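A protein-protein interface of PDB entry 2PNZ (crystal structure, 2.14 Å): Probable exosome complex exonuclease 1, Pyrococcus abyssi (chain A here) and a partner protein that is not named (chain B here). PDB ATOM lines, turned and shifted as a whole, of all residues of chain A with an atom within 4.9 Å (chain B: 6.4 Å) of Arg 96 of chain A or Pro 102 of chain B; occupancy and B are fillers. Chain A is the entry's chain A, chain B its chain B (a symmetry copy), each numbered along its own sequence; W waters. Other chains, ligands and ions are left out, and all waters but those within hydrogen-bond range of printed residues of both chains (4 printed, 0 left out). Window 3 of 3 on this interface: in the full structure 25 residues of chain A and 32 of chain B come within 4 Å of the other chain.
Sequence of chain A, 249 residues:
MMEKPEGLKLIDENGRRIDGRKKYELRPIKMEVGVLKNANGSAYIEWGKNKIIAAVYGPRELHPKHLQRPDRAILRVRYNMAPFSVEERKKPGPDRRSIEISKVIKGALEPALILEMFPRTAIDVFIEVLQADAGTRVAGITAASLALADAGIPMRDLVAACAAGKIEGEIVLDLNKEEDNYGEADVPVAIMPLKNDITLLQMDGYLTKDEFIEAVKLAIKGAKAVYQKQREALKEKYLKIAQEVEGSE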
ATOM      1  N   PRO A  94       6.171 -14.877 -26.273  1.00  0.00           N
ATOM      2  CA  PRO A  94       7.267 -15.834 -26.329  1.00  0.00           C
ATOM      3  C   PRO A  94       7.117 -16.906 -27.419  1.00  0.00           C
ATOM      4  O   PRO A  94       6.066 -17.067 -28.083  1.00  0.00           O
ATOM      5  CB  PRO A  94       7.371 -16.409 -24.888  1.00  0.00           C
ATOM      6  CG  PRO A  94       6.036 -15.948 -24.138  1.00  0.00           C
ATOM      7  CD  PRO A  94       5.229 -15.097 -25.138  1.00  0.00           C
ATOM      8  N   ASP A  95       8.243 -17.585 -27.597  1.00  0.00           N
ATOM      9  CA  ASP A  95       8.387 -18.627 -28.535  1.00  0.00           C
ATOM     10  C   ASP A  95       9.218 -19.634 -27.802  1.00  0.00           C
ATOM     11  O   ASP A  95       9.592 -19.402 -26.692  1.00  0.00           O
ATOM     12  CB  ASP A  95       9.019 -18.133 -29.878  1.00  0.00           C
ATOM     13  CG  ASP A  95      10.298 -17.312 -29.696  1.00  0.00           C
ATOM     14  OD1 ASP A  95      10.824 -16.725 -30.658  1.00  0.00           O
ATOM     15  OD2 ASP A  95      10.787 -17.214 -28.606  1.00  0.00           O
ATOM     16  N   ARG A  96       9.406 -20.790 -28.417  1.00  0.00           N
ATOM     17  CA  ARG A  96      10.042 -21.927 -27.806  1.00  0.00           C
ATOM     18  C   ARG A  96      11.425 -21.552 -27.338  1.00  0.00           C
ATOM     19  O   ARG A  96      11.799 -21.840 -26.219  1.00  0.00           O
ATOM     20  CB  ARG A  96      10.059 -23.066 -28.804  1.00  0.00           C
ATOM     21  CG  ARG A  96       8.756 -23.058 -29.506  1.00  0.00           C
ATOM     22  CD  ARG A  96       8.082 -24.337 -29.683  1.00  0.00           C
ATOM     23  NE  ARG A  96       8.955 -25.507 -29.787  1.00  0.00           N
ATOM     24  CZ  ARG A  96       8.548 -26.724 -29.420  1.00  0.00           C
ATOM     25  NH1 ARG A  96       7.328 -26.871 -28.918  1.00  0.00           N
ATOM     26  NH2 ARG A  96       9.346 -27.771 -29.528  1.00  0.00           N
ATOM     27  N   ARG A  97      12.182 -20.902 -28.194  1.00  0.00           N
ATOM     28  CA  ARG A  97      13.512 -20.451 -27.781  1.00  0.00           C
ATOM     29  C   ARG A  97      13.444 -19.595 -26.522  1.00  0.00           C
ATOM     30  O   ARG A  97      14.212 -19.830 -25.605  1.00  0.00           O
ATOM     31  CB  ARG A  97      14.221 -19.668 -28.909  1.00  0.00           C
ATOM     32  CG  ARG A  97      15.664 -19.327 -28.570  1.00  0.00           C
ATOM     33  CD  ARG A  97      16.277 -18.364 -29.497  1.00  0.00           C
ATOM     34  NE  ARG A  97      16.045 -17.015 -28.999  1.00  0.00           N
ATOM     35  CZ  ARG A  97      16.995 -16.251 -28.474  1.00  0.00           C
ATOM     36  NH1 ARG A  97      16.700 -15.043 -28.040  1.00  0.00           N
ATOM     37  NH2 ARG A  97      18.245 -16.697 -28.391  1.00  0.00           N
ATOM     38  N   SER A  98      12.599 -18.562 -26.477  1.00  0.00           N
ATOM     39  CA  SER A  98      12.601 -17.690 -25.312  1.00  0.00           C
ATOM     40  C   SER A  98      12.099 -18.427 -24.069  1.00  0.00           C
ATOM     41  O   SER A  98      12.408 -18.059 -22.950  1.00  0.00           O
ATOM     42  CB  SER A  98      11.747 -16.441 -25.555  1.00  0.00           C
ATOM     43  OG  SER A  98      10.399 -16.784 -25.761  1.00  0.00           O
ATOM     44  N   ILE A  99      11.342 -19.500 -24.257  1.00  0.00           N
ATOM     45  CA  ILE A  99      10.812 -20.182 -23.106  1.00  0.00           C
ATOM     46  C   ILE A  99      11.837 -21.121 -22.530  1.00  0.00           C
ATOM     47  O   ILE A  99      11.877 -21.265 -21.326  1.00  0.00           O
ATOM     48  CB  ILE A  99       9.554 -20.931 -23.468  1.00  0.00           C
ATOM     49  CG1 ILE A  99       8.395 -19.964 -23.490  1.00  0.00           C
ATOM     50  CG2 ILE A  99       9.287 -22.076 -22.534  1.00  0.00           C
ATOM     51  CD1 ILE A  99       7.243 -20.472 -24.274  1.00  0.00           C
ATOM     52  N   GLU A 100      12.639 -21.774 -23.369  1.00  0.00           N
ATOM     53  CA  GLU A 100      13.763 -22.568 -22.865  1.00  0.00           C
ATOM     54  C   GLU A 100      14.825 -21.649 -22.236  1.00  0.00           C
ATOM     55  O   GLU A 100      15.463 -22.003 -21.245  1.00  0.00           O
ATOM     56  CB  GLU A 100      14.326 -23.477 -23.985  1.00  0.00           C
ATOM     57  CG  GLU A 100      15.533 -24.306 -23.546  1.00  0.00           C
ATOM     58  CD  GLU A 100      16.583 -24.539 -24.640  1.00  0.00           C
ATOM     59  OE1 GLU A 100      16.406 -24.181 -25.816  1.00  0.00           O
ATOM     60  OE2 GLU A 100      17.671 -25.024 -24.297  1.00  0.00           O
ATOM     61  N   THR B  85      10.523 -31.098 -34.125  1.00  0.00           N
ATOM     62  CA  THR B  85      10.475 -32.015 -32.996  1.00  0.00           C
ATOM     63  C   THR B  85       9.515 -31.410 -32.035  1.00  0.00           C
ATOM     64  O   THR B  85       9.575 -30.222 -31.735  1.00  0.00           O
ATOM     65  CB  THR B  85      11.830 -32.085 -32.283  1.00  0.00           C
ATOM     66  OG1 THR B  85      12.853 -32.206 -33.287  1.00  0.00           O
ATOM     67  CG2 THR B  85      11.869 -33.279 -31.358  1.00  0.00           C
ATOM     68  N   ASN B  86       8.546 -32.202 -31.612  1.00  0.00           N
ATOM     69  CA  ASN B  86       7.618 -31.735 -30.610  1.00  0.00           C
ATOM     70  C   ASN B  86       7.501 -32.830 -29.575  1.00  0.00           C
ATOM     71  O   ASN B  86       7.546 -34.030 -29.908  1.00  0.00           O
ATOM     72  CB  ASN B  86       6.309 -31.376 -31.286  1.00  0.00           C
ATOM     73  CG  ASN B  86       5.309 -30.893 -30.357  1.00  0.00           C
ATOM     74  OD1 ASN B  86       4.311 -31.600 -30.100  1.00  0.00           O
ATOM     75  ND2 ASN B  86       5.473 -29.675 -29.860  1.00  0.00           N
ATOM     76  N   VAL B  87       7.432 -32.424 -28.307  1.00  0.00           N
ATOM     77  CA  VAL B  87       7.258 -33.380 -27.194  1.00  0.00           C
ATOM     78  C   VAL B  87       5.926 -32.992 -26.604  1.00  0.00           C
ATOM     79  O   VAL B  87       5.742 -31.858 -26.195  1.00  0.00           O
ATOM     80  CB  VAL B  87       8.305 -33.197 -26.161  1.00  0.00           C
ATOM     81  CG1 VAL B  87       7.896 -33.954 -24.897  1.00  0.00           C
ATOM     82  CG2 VAL B  87       9.722 -33.686 -26.718  1.00  0.00           C
ATOM     83  N   GLU B  88       4.989 -33.930 -26.624  1.00  0.00           N
ATOM     84  CA  GLU B  88       3.797 -33.883 -25.832  1.00  0.00           C
ATOM     85  C   GLU B  88       3.956 -34.632 -24.525  1.00  0.00           C
ATOM     86  O   GLU B  88       4.188 -35.848 -24.496  1.00  0.00           O
ATOM     87  CB  GLU B  88       2.657 -34.512 -26.593  1.00  0.00           C
ATOM     88  CG  GLU B  88       2.286 -33.773 -27.903  1.00  0.00           C
ATOM     89  CD  GLU B  88       1.945 -32.294 -27.669  1.00  0.00           C
ATOM     90  OE1 GLU B  88       2.440 -31.417 -28.415  1.00  0.00           O
ATOM     91  OE2 GLU B  88       1.190 -31.996 -26.748  1.00  0.00           O
ATOM     92  N   GLY B 100      -2.750 -28.718 -22.411  1.00  0.00           N
ATOM     93  CA  GLY B 100      -2.453 -27.414 -23.039  1.00  0.00           C
ATOM     94  C   GLY B 100      -1.184 -27.359 -23.900  1.00  0.00           C
ATOM     95  O   GLY B 100      -0.502 -28.390 -24.116  1.00  0.00           O
ATOM     96  N   PRO B 101      -0.822 -26.144 -24.377  1.00  0.00           N
ATOM     97  CA  PRO B 101       0.311 -26.028 -25.317  1.00  0.00           C
ATOM     98  C   PRO B 101       1.600 -26.521 -24.622  1.00  0.00           C
ATOM     99  O   PRO B 101       1.582 -26.646 -23.391  1.00  0.00           O
ATOM    100  CB  PRO B 101       0.357 -24.526 -25.615  1.00  0.00           C
ATOM    101  CG  PRO B 101      -0.329 -23.882 -24.402  1.00  0.00           C
ATOM    102  CD  PRO B 101      -1.398 -24.841 -24.031  1.00  0.00           C
ATOM    103  N   PRO B 102       2.699 -26.841 -25.375  1.00  0.00           N
ATOM    104  CA  PRO B 102       3.820 -27.285 -24.521  1.00  0.00           C
ATOM    105  C   PRO B 102       4.195 -26.348 -23.354  1.00  0.00           C
ATOM    106  O   PRO B 102       4.142 -25.094 -23.478  1.00  0.00           O
ATOM    107  CB  PRO B 102       4.980 -27.477 -25.516  1.00  0.00           C
ATOM    108  CG  PRO B 102       4.353 -27.947 -26.767  1.00  0.00           C
ATOM    109  CD  PRO B 102       3.084 -26.932 -26.802  1.00  0.00           C
ATOM    110  N   ASP B 103       4.523 -26.945 -22.204  1.00  0.00           N
ATOM    111  CA  ASP B 103       5.096 -26.150 -21.148  1.00  0.00           C
ATOM    112  C   ASP B 103       6.620 -26.087 -21.346  1.00  0.00           C
ATOM    113  O   ASP B 103       7.135 -26.651 -22.289  1.00  0.00           O
ATOM    114  CB  ASP B 103       4.713 -26.712 -19.787  1.00  0.00           C
ATOM    115  CG  ASP B 103       5.442 -28.003 -19.448  1.00  0.00           C
ATOM    116  OD1 ASP B 103       5.675 -28.853 -20.322  1.00  0.00           O
ATOM    117  OD2 ASP B 103       5.739 -28.174 -18.261  1.00  0.00           O
ATOM    118  N   GLU B 104       7.317 -25.388 -20.465  1.00  0.00           N
ATOM    119  CA  GLU B 104       8.738 -25.154 -20.596  1.00  0.00           C
ATOM    120  C   GLU B 104       9.478 -26.483 -20.511  1.00  0.00           C
ATOM    121  O   GLU B 104      10.521 -26.635 -21.123  1.00  0.00           O
ATOM    122  CB  GLU B 104       9.237 -24.151 -19.534  1.00  0.00           C
ATOM    123  CG  GLU B 104       9.123 -24.684 -18.087  1.00  0.00           C
ATOM    124  CD  GLU B 104       9.715 -23.796 -16.978  1.00  0.00           C
ATOM    125  OE1 GLU B 104      10.047 -22.617 -17.220  1.00  0.00           O
ATOM    126  OE2 GLU B 104       9.878 -24.307 -15.831  1.00  0.00           O
ATOM    127  N   ARG B 105       8.948 -27.465 -19.775  1.00  0.00           N
ATOM    128  CA  ARG B 105       9.605 -28.801 -19.732  1.00  0.00           C
ATOM    129  C   ARG B 105       9.500 -29.493 -21.094  1.00  0.00           C
ATOM    130  O   ARG B 105      10.477 -30.026 -21.602  1.00  0.00           O
ATOM    131  CB  ARG B 105       9.043 -29.716 -18.630  1.00  0.00           C
ATOM    132  CG  ARG B 105       8.945 -29.089 -17.234  1.00  0.00           C
ATOM    133  CD  ARG B 105       8.115 -29.986 -16.294  1.00  0.00           C
ATOM    134  NE  ARG B 105       6.703 -29.961 -16.691  1.00  0.00           N
ATOM    135  CZ  ARG B 105       5.682 -30.510 -16.043  1.00  0.00           C
ATOM    136  NH1 ARG B 105       5.861 -31.189 -14.904  1.00  0.00           N
ATOM    137  NH2 ARG B 105       4.455 -30.345 -16.533  1.00  0.00           N
ATOM    138  N   ALA B 106       8.338 -29.416 -21.713  1.00  0.00           N
ATOM    139  CA  ALA B 106       8.156 -30.089 -22.953  1.00  0.00           C
ATOM    140  C   ALA B 106       8.986 -29.372 -23.983  1.00  0.00           C
ATOM    141  O   ALA B 106       9.631 -30.013 -24.816  1.00  0.00           O
ATOM    142  CB  ALA B 106       6.688 -30.046 -23.340  1.00  0.00           C
ATOM    143  N   ILE B 107       8.963 -28.038 -23.940  1.00  0.00           N
ATOM    144  CA  ILE B 107       9.718 -27.247 -24.886  1.00  0.00           C
ATOM    145  C   ILE B 107      11.220 -27.470 -24.726  1.00  0.00           C
ATOM    146  O   ILE B 107      11.941 -27.577 -25.748  1.00  0.00           O
ATOM    147  CB  ILE B 107       9.337 -25.726 -24.797  1.00  0.00           C
ATOM    148  CG1 ILE B 107       7.959 -25.575 -25.435  1.00  0.00           C
ATOM    149  CG2 ILE B 107      10.421 -24.877 -25.467  1.00  0.00           C
ATOM    150  CD1 ILE B 107       7.131 -24.297 -25.204  1.00  0.00           C
ATOM    151  N   GLU B 108      11.719 -27.566 -23.503  1.00  0.00           N
ATOM    152  CA  GLU B 108      13.174 -27.852 -23.380  1.00  0.00           C
ATOM    153  C   GLU B 108      13.528 -29.243 -23.814  1.00  0.00           C
ATOM    154  O   GLU B 108      14.588 -29.451 -24.450  1.00  0.00           O
ATOM    155  CB  GLU B 108      13.697 -27.539 -21.951  1.00  0.00           C
ATOM    156  CG  GLU B 108      15.105 -28.073 -21.603  1.00  0.00           C
ATOM    157  CD  GLU B 108      15.271 -28.021 -20.139  1.00  0.00           C
ATOM    158  OE1 GLU B 108      16.215 -27.333 -19.711  1.00  0.00           O
ATOM    159  OE2 GLU B 108      14.374 -28.548 -19.412  1.00  0.00           O
ATOM    160  N   ALA B 110      11.992 -30.960 -26.179  1.00  0.00           N
ATOM    161  CA  ALA B 110      11.897 -31.041 -27.635  1.00  0.00           C
ATOM    162  C   ALA B 110      13.129 -30.389 -28.227  1.00  0.00           C
ATOM    163  O   ALA B 110      13.749 -30.954 -29.034  1.00  0.00           O
ATOM    164  CB  ALA B 110      10.639 -30.399 -28.099  1.00  0.00           C
ATOM    165  N   ARG B 111      13.545 -29.247 -27.703  1.00  0.00           N
ATOM    166  CA  ARG B 111      14.599 -28.484 -28.263  1.00  0.00           C
ATOM    167  C   ARG B 111      15.915 -29.167 -28.095  1.00  0.00           C
ATOM    168  O   ARG B 111      16.677 -29.173 -29.006  1.00  0.00           O
ATOM    169  CB  ARG B 111      14.591 -27.014 -27.754  1.00  0.00           C
ATOM    170  CG  ARG B 111      13.426 -26.277 -28.283  1.00  0.00           C
ATOM    171  CD  ARG B 111      13.271 -24.850 -27.738  1.00  0.00           C
ATOM    172  NE  ARG B 111      14.512 -24.087 -27.748  1.00  0.00           N
ATOM    173  CZ  ARG B 111      14.976 -23.488 -28.839  1.00  0.00           C
ATOM    174  NH1 ARG B 111      14.303 -23.571 -29.947  1.00  0.00           N
ATOM    175  NH2 ARG B 111      16.075 -22.774 -28.810  1.00  0.00           N
HETATM  176  O   HOH W   1       7.535 -29.509 -27.188  1.00  0.00           O
HETATM  177  O   HOH W   2      11.683 -28.205 -30.927  1.00  0.00           O
HETATM  178  O   HOH W   3       9.851 -20.990 -19.262  1.00  0.00           O
HETATM  179  O   HOH W   4       8.120 -27.705 -32.626  1.00  0.00           O
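Arg 96 of chain A touches just these residues of chain B: Thr 85, Asn 86, Pro 102, Ile 107, Ala 110 and Arg 111. Of the printed residues of chain B, Arg 97 of chain A touches Arg 111 (3.5 Å). Printed residues of chain B within 4 Å of Ile 99 of chain A: Glu 104 and Ile 107. Of the printed residues of chain A, Thr 85 of chain B touches Arg 96. Glu 88 of chain B touches none of the printed residues of chain A. Printed residues of chain A within 4 Å of Pro 102 of chain B: Arg 96. Of the printed residues of chain A, Glu 104 of chain B touches Ile 99 (3.6 Å). Printed residues of chain A within 4 Å of Ala 110 of chain B: Arg 96.
The backbone carbonyl oxygen (O) of Thr 85 of chain B is in hydrogen-bond range of the guanidinium group (NH2) of Arg 96 of chain A (3.3 Å). NH1 of Arg 96 of chain A lies close to ND2 of Asn 86 of chain B, 3.5 Å away. NE of Arg 111 of chain B is in salt-bridge range of OE1 of Glu 100 of chain A.
Among the printed residues, merely in contact across the chains: Arg 96 of chain A with Pro 102 of chain B (3.8 Å), Arg 96 of chain A with Ile 107 of chain B (3.4 Å), Arg 96 of chain A with Ala 110 of chain B (3.3 Å), Arg 96 of chain A with Arg 111 of chain B (3.7 Å), Arg 97 of chain A with Arg 111 of chain B (3.5 Å), Ile 99 of chain A with Glu 104 of chain B (3.6 Å) and Ile 99 of chain A with Ile 107 of chain B (3.9 Å).
Water W3 lies within hydrogen-bond range of the side-chain carboxylate of Glu 104 of chain B (2.6 Å) and the backbone carbonyl oxygen of Ile 99 of chain A (2.9 Å). Water W2 bridges NH2 of Arg 96 of chain A (2.8 Å) and O of Thr 85 of chain B (3.0 Å). Water W4 lies within hydrogen-bond range of O of Thr 85 of chain B and NH2 of Arg 96 of chain A. Water W1 lies within hydrogen-bond range of O of Val 87 of chain B, NH1 of Arg 96 of chain A, O of Ala 106 of chain B and ND2 of Asn 86 of chain B.
OD1 of Asn 86 of chain B lies close to OE1 of Glu 88 of chain B (2.5 Å).
Hydrophobic or aromatic side chains of chain B that line the printed part of chain A: Pro 102, Ile 107 and Ala 110. Among the printed residues, Asp or Glu carboxylates within 4 Å of a Lys or Arg side-chain nitrogen of the other chain: Glu 100 of chain A with Arg 111 of chain B (2.7 Å).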
